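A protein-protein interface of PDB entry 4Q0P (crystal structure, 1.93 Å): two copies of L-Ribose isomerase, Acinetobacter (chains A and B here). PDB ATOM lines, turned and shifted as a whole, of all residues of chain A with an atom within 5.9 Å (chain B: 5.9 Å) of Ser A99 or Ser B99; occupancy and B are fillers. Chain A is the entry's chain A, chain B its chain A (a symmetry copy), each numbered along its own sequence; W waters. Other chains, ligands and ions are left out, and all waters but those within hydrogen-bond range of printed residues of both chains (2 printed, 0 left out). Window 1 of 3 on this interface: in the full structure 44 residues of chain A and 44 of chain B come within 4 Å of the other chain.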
ATOM      1  N   GLU A  82      19.745 -11.737  17.820  1.00  0.00           N
ATOM      2  CA  GLU A  82      19.416 -11.139  19.096  1.00  0.00           C
ATOM      3  C   GLU A  82      19.080  -9.649  18.997  1.00  0.00           C
ATOM      4  O   GLU A  82      19.917  -8.838  18.604  1.00  0.00           O
ATOM      5  CB  GLU A  82      20.599 -11.352  20.046  1.00  0.00           C
ATOM      6  CG  GLU A  82      20.546 -10.550  21.324  1.00  0.00           C
ATOM      7  CD  GLU A  82      19.280 -10.803  22.115  1.00  0.00           C
ATOM      8  OE1 GLU A  82      18.867 -11.981  22.221  1.00  0.00           O
ATOM      9  OE2 GLU A  82      18.711  -9.819  22.637  1.00  0.00           O
ATOM     10  N   PRO A  83      17.846  -9.277  19.364  1.00  0.00           N
ATOM     11  CA  PRO A  83      17.386  -7.884  19.325  1.00  0.00           C
ATOM     12  C   PRO A  83      18.294  -6.947  20.117  1.00  0.00           C
ATOM     13  O   PRO A  83      18.537  -5.810  19.709  1.00  0.00           O
ATOM     14  CB  PRO A  83      15.988  -7.968  19.937  1.00  0.00           C
ATOM     15  CG  PRO A  83      15.531  -9.339  19.544  1.00  0.00           C
ATOM     16  CD  PRO A  83      16.758 -10.175  19.798  1.00  0.00           C
ATOM     17  N   ALA A  84      18.793  -7.433  21.252  1.00  0.00           N
ATOM     18  CA  ALA A  84      19.657  -6.645  22.131  1.00  0.00           C
ATOM     19  C   ALA A  84      18.906  -5.420  22.656  1.00  0.00           C
ATOM     20  O   ALA A  84      19.480  -4.333  22.798  1.00  0.00           O
ATOM     21  CB  ALA A  84      20.919  -6.213  21.396  1.00  0.00           C
ATOM     22  N   TYR A  95      15.609   3.618  17.717  1.00  0.00           N
ATOM     23  CA  TYR A  95      16.879   3.357  17.049  1.00  0.00           C
ATOM     24  C   TYR A  95      17.402   1.946  17.299  1.00  0.00           C
ATOM     25  O   TYR A  95      18.445   1.564  16.767  1.00  0.00           O
ATOM     26  CB  TYR A  95      17.926   4.376  17.507  1.00  0.00           C
ATOM     27  CG  TYR A  95      17.460   5.805  17.361  1.00  0.00           C
ATOM     28  CD1 TYR A  95      17.178   6.340  16.104  1.00  0.00           C
ATOM     29  CD2 TYR A  95      17.258   6.610  18.482  1.00  0.00           C
ATOM     30  CE1 TYR A  95      16.703   7.641  15.964  1.00  0.00           C
ATOM     31  CE2 TYR A  95      16.783   7.915  18.354  1.00  0.00           C
ATOM     32  CZ  TYR A  95      16.507   8.422  17.093  1.00  0.00           C
ATOM     33  OH  TYR A  95      16.027   9.703  16.956  1.00  0.00           O
ATOM     34  N   ALA A  96      16.673   1.175  18.096  1.00  0.00           N
ATOM     35  CA  ALA A  96      17.080  -0.189  18.427  1.00  0.00           C
ATOM     36  C   ALA A  96      17.184  -1.095  17.202  1.00  0.00           C
ATOM     37  O   ALA A  96      18.024  -1.992  17.157  1.00  0.00           O
ATOM     38  CB  ALA A  96      16.105  -0.789  19.437  1.00  0.00           C
ATOM     39  N   GLU A  97      16.326  -0.847  16.216  1.00  0.00           N
ATOM     40  CA  GLU A  97      16.283  -1.627  14.984  1.00  0.00           C
ATOM     41  C   GLU A  97      17.595  -1.609  14.196  1.00  0.00           C
ATOM     42  O   GLU A  97      17.800  -2.433  13.304  1.00  0.00           O
ATOM     43  CB  GLU A  97      15.137  -1.118  14.103  1.00  0.00           C
ATOM     44  CG  GLU A  97      15.279   0.340  13.686  1.00  0.00           C
ATOM     45  CD  GLU A  97      13.950   0.976  13.321  1.00  0.00           C
ATOM     46  OE1 GLU A  97      13.102   1.129  14.224  1.00  0.00           O
ATOM     47  OE2 GLU A  97      13.752   1.317  12.136  1.00  0.00           O
ATOM     48  N   TYR A  98      18.476  -0.671  14.521  1.00  0.00           N
ATOM     49  CA  TYR A  98      19.766  -0.561  13.842  1.00  0.00           C
ATOM     50  C   TYR A  98      20.847  -1.377  14.548  1.00  0.00           C
ATOM     51  O   TYR A  98      21.939  -1.564  14.015  1.00  0.00           O
ATOM     52  CB  TYR A  98      20.209   0.904  13.783  1.00  0.00           C
ATOM     53  CG  TYR A  98      19.355   1.768  12.893  1.00  0.00           C
ATOM     54  CD1 TYR A  98      19.545   1.782  11.510  1.00  0.00           C
ATOM     55  CD2 TYR A  98      18.341   2.568  13.428  1.00  0.00           C
ATOM     56  CE1 TYR A  98      18.750   2.569  10.684  1.00  0.00           C
ATOM     57  CE2 TYR A  98      17.538   3.358  12.608  1.00  0.00           C
ATOM     58  CZ  TYR A  98      17.750   3.353  11.238  1.00  0.00           C
ATOM     59  OH  TYR A  98      16.961   4.128  10.424  1.00  0.00           O
ATOM     60  N   SER A  99      20.539  -1.857  15.750  1.00  0.00           N
ATOM     61  CA  SER A  99      21.492  -2.640  16.523  1.00  0.00           C
ATOM     62  C   SER A  99      21.113  -4.122  16.540  1.00  0.00           C
ATOM     63  O   SER A  99      20.523  -4.633  15.585  1.00  0.00           O
ATOM     64  CB  SER A  99      21.575  -2.098  17.956  1.00  0.00           C
ATOM     65  OG  SER A  99      22.623  -2.716  18.690  1.00  0.00           O
ATOM     66  N   GLY A 100      21.446  -4.806  17.630  1.00  0.00           N
ATOM     67  CA  GLY A 100      21.147  -6.225  17.726  1.00  0.00           C
ATOM     68  C   GLY A 100      22.335  -7.020  17.209  1.00  0.00           C
ATOM     69  O   GLY A 100      23.313  -6.438  16.746  1.00  0.00           O
ATOM     70  N   LEU A 101      22.255  -8.344  17.276  1.00  0.00           N
ATOM     71  CA  LEU A 101      23.350  -9.200  16.823  1.00  0.00           C
ATOM     72  C   LEU A 101      22.848 -10.404  16.039  1.00  0.00           C
ATOM     73  O   LEU A 101      22.075 -11.210  16.554  1.00  0.00           O
ATOM     74  CB  LEU A 101      24.155  -9.683  18.028  1.00  0.00           C
ATOM     75  CG  LEU A 101      24.835  -8.583  18.844  1.00  0.00           C
ATOM     76  CD1 LEU A 101      25.302  -9.142  20.188  1.00  0.00           C
ATOM     77  CD2 LEU A 101      25.995  -8.008  18.049  1.00  0.00           C
ATOM     78  N   ARG A 121      18.854  -0.609   7.714  1.00  0.00           N
ATOM     79  CA  ARG A 121      19.294  -0.722   9.105  1.00  0.00           C
ATOM     80  C   ARG A 121      20.481  -1.640   9.369  1.00  0.00           C
ATOM     81  O   ARG A 121      21.355  -1.320  10.181  1.00  0.00           O
ATOM     82  CB  ARG A 121      18.116  -1.186   9.962  1.00  0.00           C
ATOM     83  CG  ARG A 121      16.814  -0.478   9.625  1.00  0.00           C
ATOM     84  CD  ARG A 121      15.634  -1.113  10.335  1.00  0.00           C
ATOM     85  NE  ARG A 121      14.362  -0.499   9.959  1.00  0.00           N
ATOM     86  CZ  ARG A 121      13.825  -0.567   8.744  1.00  0.00           C
ATOM     87  NH1 ARG A 121      14.448  -1.224   7.772  1.00  0.00           N
ATOM     88  NH2 ARG A 121      12.661   0.021   8.498  1.00  0.00           N
ATOM     89  N   ARG A 195      25.452  -0.385   6.327  1.00  0.00           N
ATOM     90  CA  ARG A 195      24.051  -0.340   5.930  1.00  0.00           C
ATOM     91  C   ARG A 195      23.918   0.751   4.860  1.00  0.00           C
ATOM     92  O   ARG A 195      24.778   1.620   4.756  1.00  0.00           O
ATOM     93  CB  ARG A 195      23.176   0.003   7.141  1.00  0.00           C
ATOM     94  CG  ARG A 195      23.583   1.291   7.845  1.00  0.00           C
ATOM     95  CD  ARG A 195      22.616   1.650   8.958  1.00  0.00           C
ATOM     96  NE  ARG A 195      22.785   0.820  10.149  1.00  0.00           N
ATOM     97  CZ  ARG A 195      23.725   1.017  11.067  1.00  0.00           C
ATOM     98  NH1 ARG A 195      24.587   2.016  10.932  1.00  0.00           N
ATOM     99  NH2 ARG A 195      23.788   0.226  12.133  1.00  0.00           N
ATOM    100  N   THR A 218      24.214  -6.620  12.409  1.00  0.00           N
ATOM    101  CA  THR A 218      23.242  -6.145  13.376  1.00  0.00           C
ATOM    102  C   THR A 218      21.972  -6.951  13.094  1.00  0.00           C
ATOM    103  O   THR A 218      21.940  -7.747  12.145  1.00  0.00           O
ATOM    104  CB  THR A 218      22.995  -4.623  13.219  1.00  0.00           C
ATOM    105  OG1 THR A 218      22.683  -4.315  11.854  1.00  0.00           O
ATOM    106  CG2 THR A 218      24.239  -3.847  13.627  1.00  0.00           C
ATOM    107  N   TYR A 219      20.936  -6.753  13.904  1.00  0.00           N
ATOM    108  CA  TYR A 219      19.689  -7.498  13.759  1.00  0.00           C
ATOM    109  C   TYR A 219      19.188  -7.589  12.323  1.00  0.00           C
ATOM    110  O   TYR A 219      19.259  -6.624  11.567  1.00  0.00           O
ATOM    111  CB  TYR A 219      18.600  -6.875  14.634  1.00  0.00           C
ATOM    112  CG  TYR A 219      17.397  -7.764  14.840  1.00  0.00           C
ATOM    113  CD1 TYR A 219      17.415  -8.783  15.797  1.00  0.00           C
ATOM    114  CD2 TYR A 219      16.234  -7.585  14.092  1.00  0.00           C
ATOM    115  CE1 TYR A 219      16.302  -9.599  16.008  1.00  0.00           C
ATOM    116  CE2 TYR A 219      15.112  -8.396  14.296  1.00  0.00           C
ATOM    117  CZ  TYR A 219      15.157  -9.398  15.257  1.00  0.00           C
ATOM    118  OH  TYR A 219      14.053 -10.189  15.475  1.00  0.00           O
ATOM    119  N   SER A 220      18.658  -8.752  11.964  1.00  0.00           N
ATOM    120  CA  SER A 220      18.142  -8.974  10.624  1.00  0.00           C
ATOM    121  C   SER A 220      16.617  -8.988  10.646  1.00  0.00           C
ATOM    122  O   SER A 220      15.999  -9.965  11.071  1.00  0.00           O
ATOM    123  CB  SER A 220      18.679 -10.297  10.071  1.00  0.00           C
ATOM    124  OG  SER A 220      18.238 -10.514   8.741  1.00  0.00           O
ATOM    125  N   HIS A 221      16.017  -7.890  10.196  1.00  0.00           N
ATOM    126  CA  HIS A 221      14.563  -7.748  10.153  1.00  0.00           C
ATOM    127  C   HIS A 221      14.002  -8.481   8.939  1.00  0.00           C
ATOM    128  O   HIS A 221      14.108  -7.999   7.813  1.00  0.00           O
ATOM    129  CB  HIS A 221      14.189  -6.268  10.078  1.00  0.00           C
ATOM    130  CG  HIS A 221      14.710  -5.458  11.222  1.00  0.00           C
ATOM    131  ND1 HIS A 221      14.082  -5.412  12.448  1.00  0.00           N
ATOM    132  CD2 HIS A 221      15.818  -4.688  11.337  1.00  0.00           C
ATOM    133  CE1 HIS A 221      14.781  -4.648  13.270  1.00  0.00           C
ATOM    134  NE2 HIS A 221      15.840  -4.197  12.621  1.00  0.00           N
ATOM    135  N   TRP A 237       9.089  -2.866  15.180  1.00  0.00           N
ATOM    136  CA  TRP A 237       9.744  -4.023  14.576  1.00  0.00           C
ATOM    137  C   TRP A 237       8.792  -5.008  13.904  1.00  0.00           C
ATOM    138  O   TRP A 237       9.166  -5.671  12.939  1.00  0.00           O
ATOM    139  CB  TRP A 237      10.564  -4.761  15.636  1.00  0.00           C
ATOM    140  CG  TRP A 237      11.744  -3.990  16.152  1.00  0.00           C
ATOM    141  CD1 TRP A 237      11.819  -2.642  16.358  1.00  0.00           C
ATOM    142  CD2 TRP A 237      12.996  -4.533  16.583  1.00  0.00           C
ATOM    143  NE1 TRP A 237      13.040  -2.312  16.896  1.00  0.00           N
ATOM    144  CE2 TRP A 237      13.781  -3.455  17.046  1.00  0.00           C
ATOM    145  CE3 TRP A 237      13.529  -5.829  16.630  1.00  0.00           C
ATOM    146  CZ2 TRP A 237      15.074  -3.631  17.549  1.00  0.00           C
ATOM    147  CZ3 TRP A 237      14.814  -6.003  17.131  1.00  0.00           C
ATOM    148  CH2 TRP A 237      15.571  -4.909  17.585  1.00  0.00           C
ATOM    149  N   GLU B  82      33.595  -2.755  15.190  1.00  0.00           N
ATOM    150  CA  GLU B  82      32.990  -1.804  14.282  1.00  0.00           C
ATOM    151  C   GLU B  82      31.909  -0.944  14.940  1.00  0.00           C
ATOM    152  O   GLU B  82      30.891  -1.455  15.404  1.00  0.00           O
ATOM    153  CB  GLU B  82      32.402  -2.578  13.097  1.00  0.00           C
ATOM    154  CG  GLU B  82      31.489  -1.777  12.200  1.00  0.00           C
ATOM    155  CD  GLU B  82      32.161  -0.541  11.643  1.00  0.00           C
ATOM    156  OE1 GLU B  82      33.341  -0.634  11.234  1.00  0.00           O
ATOM    157  OE2 GLU B  82      31.497   0.519  11.608  1.00  0.00           O
ATOM    158  N   PRO B  83      32.120   0.378  14.976  1.00  0.00           N
ATOM    159  CA  PRO B  83      31.169   1.325  15.572  1.00  0.00           C
ATOM    160  C   PRO B  83      29.769   1.201  14.973  1.00  0.00           C
ATOM    161  O   PRO B  83      28.768   1.321  15.680  1.00  0.00           O
ATOM    162  CB  PRO B  83      31.798   2.682  15.263  1.00  0.00           C
ATOM    163  CG  PRO B  83      33.265   2.380  15.258  1.00  0.00           C
ATOM    164  CD  PRO B  83      33.325   1.082  14.496  1.00  0.00           C
ATOM    165  N   ALA B  84      29.711   0.959  13.665  1.00  0.00           N
ATOM    166  CA  ALA B  84      28.442   0.841  12.945  1.00  0.00           C
ATOM    167  C   ALA B  84      27.661   2.154  13.025  1.00  0.00           C
ATOM    168  O   ALA B  84      26.429   2.158  13.141  1.00  0.00           O
ATOM    169  CB  ALA B  84      27.608  -0.302  13.511  1.00  0.00           C
ATOM    170  N   TYR B  95      22.589   6.986  21.263  1.00  0.00           N
ATOM    171  CA  TYR B  95      22.327   5.578  21.533  1.00  0.00           C
ATOM    172  C   TYR B  95      23.220   4.641  20.726  1.00  0.00           C
ATOM    173  O   TYR B  95      23.144   3.422  20.876  1.00  0.00           O
ATOM    174  CB  TYR B  95      20.859   5.257  21.242  1.00  0.00           C
ATOM    175  CG  TYR B  95      19.901   6.187  21.949  1.00  0.00           C
ATOM    176  CD1 TYR B  95      19.839   6.224  23.342  1.00  0.00           C
ATOM    177  CD2 TYR B  95      19.090   7.062  21.228  1.00  0.00           C
ATOM    178  CE1 TYR B  95      18.993   7.111  24.002  1.00  0.00           C
ATOM    179  CE2 TYR B  95      18.239   7.955  21.878  1.00  0.00           C
ATOM    180  CZ  TYR B  95      18.198   7.974  23.265  1.00  0.00           C
ATOM    181  OH  TYR B  95      17.371   8.858  23.917  1.00  0.00           O
ATOM    182  N   ALA B  96      24.070   5.213  19.881  1.00  0.00           N
ATOM    183  CA  ALA B  96      24.963   4.422  19.037  1.00  0.00           C
ATOM    184  C   ALA B  96      25.929   3.554  19.840  1.00  0.00           C
ATOM    185  O   ALA B  96      26.291   2.460  19.411  1.00  0.00           O
ATOM    186  CB  ALA B  96      25.744   5.344  18.104  1.00  0.00           C
ATOM    187  N   GLU B  97      26.337   4.054  21.004  1.00  0.00           N
ATOM    188  CA  GLU B  97      27.268   3.360  21.885  1.00  0.00           C
ATOM    189  C   GLU B  97      26.774   1.988  22.351  1.00  0.00           C
ATOM    190  O   GLU B  97      27.554   1.180  22.855  1.00  0.00           O
ATOM    191  CB  GLU B  97      27.573   4.245  23.098  1.00  0.00           C
ATOM    192  CG  GLU B  97      26.349   4.579  23.941  1.00  0.00           C
ATOM    193  CD  GLU B  97      26.531   5.846  24.759  1.00  0.00           C
ATOM    194  OE1 GLU B  97      26.632   6.931  24.151  1.00  0.00           O
ATOM    195  OE2 GLU B  97      26.577   5.757  26.004  1.00  0.00           O
ATOM    196  N   TYR B  98      25.481   1.731  22.188  1.00  0.00           N
ATOM    197  CA  TYR B  98      24.896   0.453  22.589  1.00  0.00           C
ATOM    198  C   TYR B  98      24.920  -0.561  21.448  1.00  0.00           C
ATOM    199  O   TYR B  98      24.653  -1.744  21.655  1.00  0.00           O
ATOM    200  CB  TYR B  98      23.448   0.655  23.044  1.00  0.00           C
ATOM    201  CG  TYR B  98      23.310   1.435  24.326  1.00  0.00           C
ATOM    202  CD1 TYR B  98      23.485   0.816  25.564  1.00  0.00           C
ATOM    203  CD2 TYR B  98      23.016   2.801  24.306  1.00  0.00           C
ATOM    204  CE1 TYR B  98      23.371   1.535  26.750  1.00  0.00           C
ATOM    205  CE2 TYR B  98      22.903   3.530  25.488  1.00  0.00           C
ATOM    206  CZ  TYR B  98      23.080   2.890  26.704  1.00  0.00           C
ATOM    207  OH  TYR B  98      22.971   3.604  27.872  1.00  0.00           O
ATOM    208  N   SER B  99      25.235  -0.093  20.243  1.00  0.00           N
ATOM    209  CA  SER B  99      25.279  -0.963  19.077  1.00  0.00           C
ATOM    210  C   SER B  99      26.719  -1.240  18.641  1.00  0.00           C
ATOM    211  O   SER B  99      27.634  -1.267  19.469  1.00  0.00           O
ATOM    212  CB  SER B  99      24.488  -0.332  17.923  1.00  0.00           C
ATOM    213  OG  SER B  99      24.354  -1.229  16.828  1.00  0.00           O
ATOM    214  N   GLY B 100      26.917  -1.436  17.342  1.00  0.00           N
ATOM    215  CA  GLY B 100      28.249  -1.729  16.839  1.00  0.00           C
ATOM    216  C   GLY B 100      28.450  -3.236  16.808  1.00  0.00           C
ATOM    217  O   GLY B 100      27.572  -3.984  17.231  1.00  0.00           O
ATOM    218  N   LEU B 101      29.600  -3.685  16.320  1.00  0.00           N
ATOM    219  CA  LEU B 101      29.884  -5.116  16.228  1.00  0.00           C
ATOM    220  C   LEU B 101      31.310  -5.444  16.648  1.00  0.00           C
ATOM    221  O   LEU B 101      32.267  -4.943  16.061  1.00  0.00           O
ATOM    222  CB  LEU B 101      29.659  -5.594  14.795  1.00  0.00           C
ATOM    223  CG  LEU B 101      28.228  -5.449  14.275  1.00  0.00           C
ATOM    224  CD1 LEU B 101      28.203  -5.623  12.757  1.00  0.00           C
ATOM    225  CD2 LEU B 101      27.335  -6.466  14.964  1.00  0.00           C
ATOM    226  N   ARG B 121      26.620  -0.844  28.397  1.00  0.00           N
ATOM    227  CA  ARG B 121      26.220  -0.798  26.990  1.00  0.00           C
ATOM    228  C   ARG B 121      26.368  -2.092  26.200  1.00  0.00           C
ATOM    229  O   ARG B 121      25.506  -2.432  25.383  1.00  0.00           O
ATOM    230  CB  ARG B 121      27.016   0.300  26.284  1.00  0.00           C
ATOM    231  CG  ARG B 121      27.117   1.582  27.094  1.00  0.00           C
ATOM    232  CD  ARG B 121      28.088   2.564  26.467  1.00  0.00           C
ATOM    233  NE  ARG B 121      28.262   3.769  27.275  1.00  0.00           N
ATOM    234  CZ  ARG B 121      28.827   3.790  28.480  1.00  0.00           C
ATOM    235  NH1 ARG B 121      29.279   2.667  29.028  1.00  0.00           N
ATOM    236  NH2 ARG B 121      28.946   4.936  29.138  1.00  0.00           N
ATOM    237  N   ARG B 195      23.493  -6.821  28.415  1.00  0.00           N
ATOM    238  CA  ARG B 195      24.218  -5.746  29.079  1.00  0.00           C
ATOM    239  C   ARG B 195      23.573  -5.547  30.456  1.00  0.00           C
ATOM    240  O   ARG B 195      22.436  -5.958  30.669  1.00  0.00           O
ATOM    241  CB  ARG B 195      24.109  -4.458  28.256  1.00  0.00           C
ATOM    242  CG  ARG B 195      22.673  -4.042  27.957  1.00  0.00           C
ATOM    243  CD  ARG B 195      22.616  -2.702  27.249  1.00  0.00           C
ATOM    244  NE  ARG B 195      22.998  -2.785  25.841  1.00  0.00           N
ATOM    245  CZ  ARG B 195      22.186  -3.195  24.871  1.00  0.00           C
ATOM    246  NH1 ARG B 195      20.944  -3.566  25.156  1.00  0.00           N
ATOM    247  NH2 ARG B 195      22.612  -3.215  23.613  1.00  0.00           N
ATOM    248  N   THR B 218      28.164  -6.276  20.980  1.00  0.00           N
ATOM    249  CA  THR B 218      28.039  -4.933  20.445  1.00  0.00           C
ATOM    250  C   THR B 218      29.399  -4.277  20.692  1.00  0.00           C
ATOM    251  O   THR B 218      30.283  -4.892  21.305  1.00  0.00           O
ATOM    252  CB  THR B 218      26.899  -4.155  21.150  1.00  0.00           C
ATOM    253  OG1 THR B 218      27.064  -4.221  22.572  1.00  0.00           O
ATOM    254  CG2 THR B 218      25.550  -4.758  20.783  1.00  0.00           C
ATOM    255  N   TYR B 219      29.572  -3.045  20.222  1.00  0.00           N
ATOM    256  CA  TYR B 219      30.843  -2.339  20.358  1.00  0.00           C
ATOM    257  C   TYR B 219      31.454  -2.431  21.750  1.00  0.00           C
ATOM    258  O   TYR B 219      30.753  -2.350  22.755  1.00  0.00           O
ATOM    259  CB  TYR B 219      30.667  -0.866  19.982  1.00  0.00           C
ATOM    260  CG  TYR B 219      31.968  -0.138  19.737  1.00  0.00           C
ATOM    261  CD1 TYR B 219      32.631  -0.248  18.511  1.00  0.00           C
ATOM    262  CD2 TYR B 219      32.533   0.673  20.720  1.00  0.00           C
ATOM    263  CE1 TYR B 219      33.824   0.435  18.268  1.00  0.00           C
ATOM    264  CE2 TYR B 219      33.728   1.363  20.488  1.00  0.00           C
ATOM    265  CZ  TYR B 219      34.364   1.238  19.258  1.00  0.00           C
ATOM    266  OH  TYR B 219      35.530   1.926  19.016  1.00  0.00           O
ATOM    267  N   SER B 220      32.773  -2.575  21.799  1.00  0.00           N
ATOM    268  CA  SER B 220      33.484  -2.677  23.061  1.00  0.00           C
ATOM    269  C   SER B 220      34.235  -1.379  23.345  1.00  0.00           C
ATOM    270  O   SER B 220      35.280  -1.110  22.752  1.00  0.00           O
ATOM    271  CB  SER B 220      34.458  -3.857  23.018  1.00  0.00           C
ATOM    272  OG  SER B 220      35.126  -4.016  24.259  1.00  0.00           O
ATOM    273  N   HIS B 221      33.685  -0.573  24.248  1.00  0.00           N
ATOM    274  CA  HIS B 221      34.283   0.705  24.629  1.00  0.00           C
ATOM    275  C   HIS B 221      35.424   0.477  25.613  1.00  0.00           C
ATOM    276  O   HIS B 221      35.191   0.206  26.790  1.00  0.00           O
ATOM    277  CB  HIS B 221      33.223   1.602  25.269  1.00  0.00           C
ATOM    278  CG  HIS B 221      32.050   1.873  24.383  1.00  0.00           C
ATOM    279  ND1 HIS B 221      32.069   2.836  23.396  1.00  0.00           N
ATOM    280  CD2 HIS B 221      30.833   1.285  24.310  1.00  0.00           C
ATOM    281  CE1 HIS B 221      30.913   2.829  22.755  1.00  0.00           C
ATOM    282  NE2 HIS B 221      30.146   1.896  23.289  1.00  0.00           N
ATOM    283  N   TRP B 237      31.789   9.031  22.744  1.00  0.00           N
ATOM    284  CA  TRP B 237      32.574   7.799  22.780  1.00  0.00           C
ATOM    285  C   TRP B 237      34.011   7.981  23.261  1.00  0.00           C
ATOM    286  O   TRP B 237      34.587   7.070  23.851  1.00  0.00           O
ATOM    287  CB  TRP B 237      32.588   7.157  21.391  1.00  0.00           C
ATOM    288  CG  TRP B 237      31.253   6.643  20.936  1.00  0.00           C
ATOM    289  CD1 TRP B 237      30.029   7.197  21.183  1.00  0.00           C
ATOM    290  CD2 TRP B 237      31.016   5.502  20.104  1.00  0.00           C
ATOM    291  NE1 TRP B 237      29.046   6.475  20.552  1.00  0.00           N
ATOM    292  CE2 TRP B 237      29.625   5.430  19.880  1.00  0.00           C
ATOM    293  CE3 TRP B 237      31.848   4.536  19.519  1.00  0.00           C
ATOM    294  CZ2 TRP B 237      29.042   4.428  19.097  1.00  0.00           C
ATOM    295  CZ3 TRP B 237      31.269   3.541  18.741  1.00  0.00           C
ATOM    296  CH2 TRP B 237      29.878   3.496  18.536  1.00  0.00           C
HETATM  297  O   HOH W   1      21.348  -2.134  21.356  1.00  0.00           O
HETATM  298  O   HOH W   2      23.942   0.984  14.827  1.00  0.00           O
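Among the printed residues, pairs that only touch across the chains: Tyr A95 with Tyr B95, Leu A101 with Leu B101, Ser A99 with Tyr B98 and Tyr A98 with Ser B99.
Of the 17 printed residues of chain A, 6 touch a printed residue of chain B. Hydrophobic or aromatic side chains of chain A within 4 Å of the printed part of chain B: Tyr A95 and Leu A101. Among the printed residues, no Asp or Glu carboxylate lies within 4 Å of a Lys or Arg side-chain nitrogen of the other chain.
The side-chain hydroxyl (OG) of Ser B99 sits at hydrogen-bond distance from the side-chain hydroxyl (OG) of Ser A99. The backbone carbonyl oxygen (O) of Ala A84 lies within hydrogen-bond range of the guanidinium group (NH1) of Arg B195 (2.9 Å). O of Ala B84 is in hydrogen-bond range of NH1 of Arg A195 (2.9 Å).
Water W1 lies within hydrogen-bond range of NH2 of Arg B195, OG of Ser A99, O of Ala A84 and O of Tyr B98. Water W2 lies within hydrogen-bond range of NH2 of Arg A195 (2.8 Å), OG of Ser B99 (3.0 Å), O of Ala B84 (3.2 Å) and O of Tyr A98 (3.3 Å).
The backbone NH of Ala A84 is in hydrogen-bond range of the side-chain carboxylate of Glu A82, at 2.8 Å. N of Tyr A219 is in hydrogen-bond range of O of Ser A99, 2.7 Å away. The backbone NH of Glu B82 lies within hydrogen-bond range of the backbone carbonyl oxygen of Leu B101 (2.7 Å). N of Tyr B219 lies within hydrogen-bond range of O of Ser B99. The guanidinium group (NH2) of Arg A195 is in hydrogen-bond range of the backbone carbonyl oxygen (O) of Tyr A98 (3.2 Å). O of Leu A101 is in hydrogen-bond range of N of Glu A82, 2.7 Å away.
Printed residues of chain B within 4 Å of Tyr A98: Ser B99 (3.7 Å). Of chain B, only Tyr B98 (3.7 Å) and Ser B99 (2.9 Å) come within 4 Å of Ser A99. Of the printed residues of chain A, Ala B84 touches Arg A195. Of the printed residues of chain A, Tyr B98 touches Ser A99. Printed residues of chain A within 4 Å of Ser B99: Tyr A98 and Ser A99. Printed residues of chain A within 4 Å of Arg B195: Ala A84. The nearest residue of chain B that does not touch Ser A99 is Thr B218 (4.1 Å). The nearest residue of chain A that does not touch Ser B99 is Thr A218 (4.1 Å). The nearest printed residue of chain B that does not touch Tyr A95 is Ser B99 (6.4 Å).
Ala A84 touches Arg B195, and with the chains exchanged Arg A195 touches Ala B84. Tyr B95 touches its own counterpart, Tyr A95. Ser B99 touches its own counterpart, Ser A99. Leu A101 touches its own counterpart, Leu B101.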
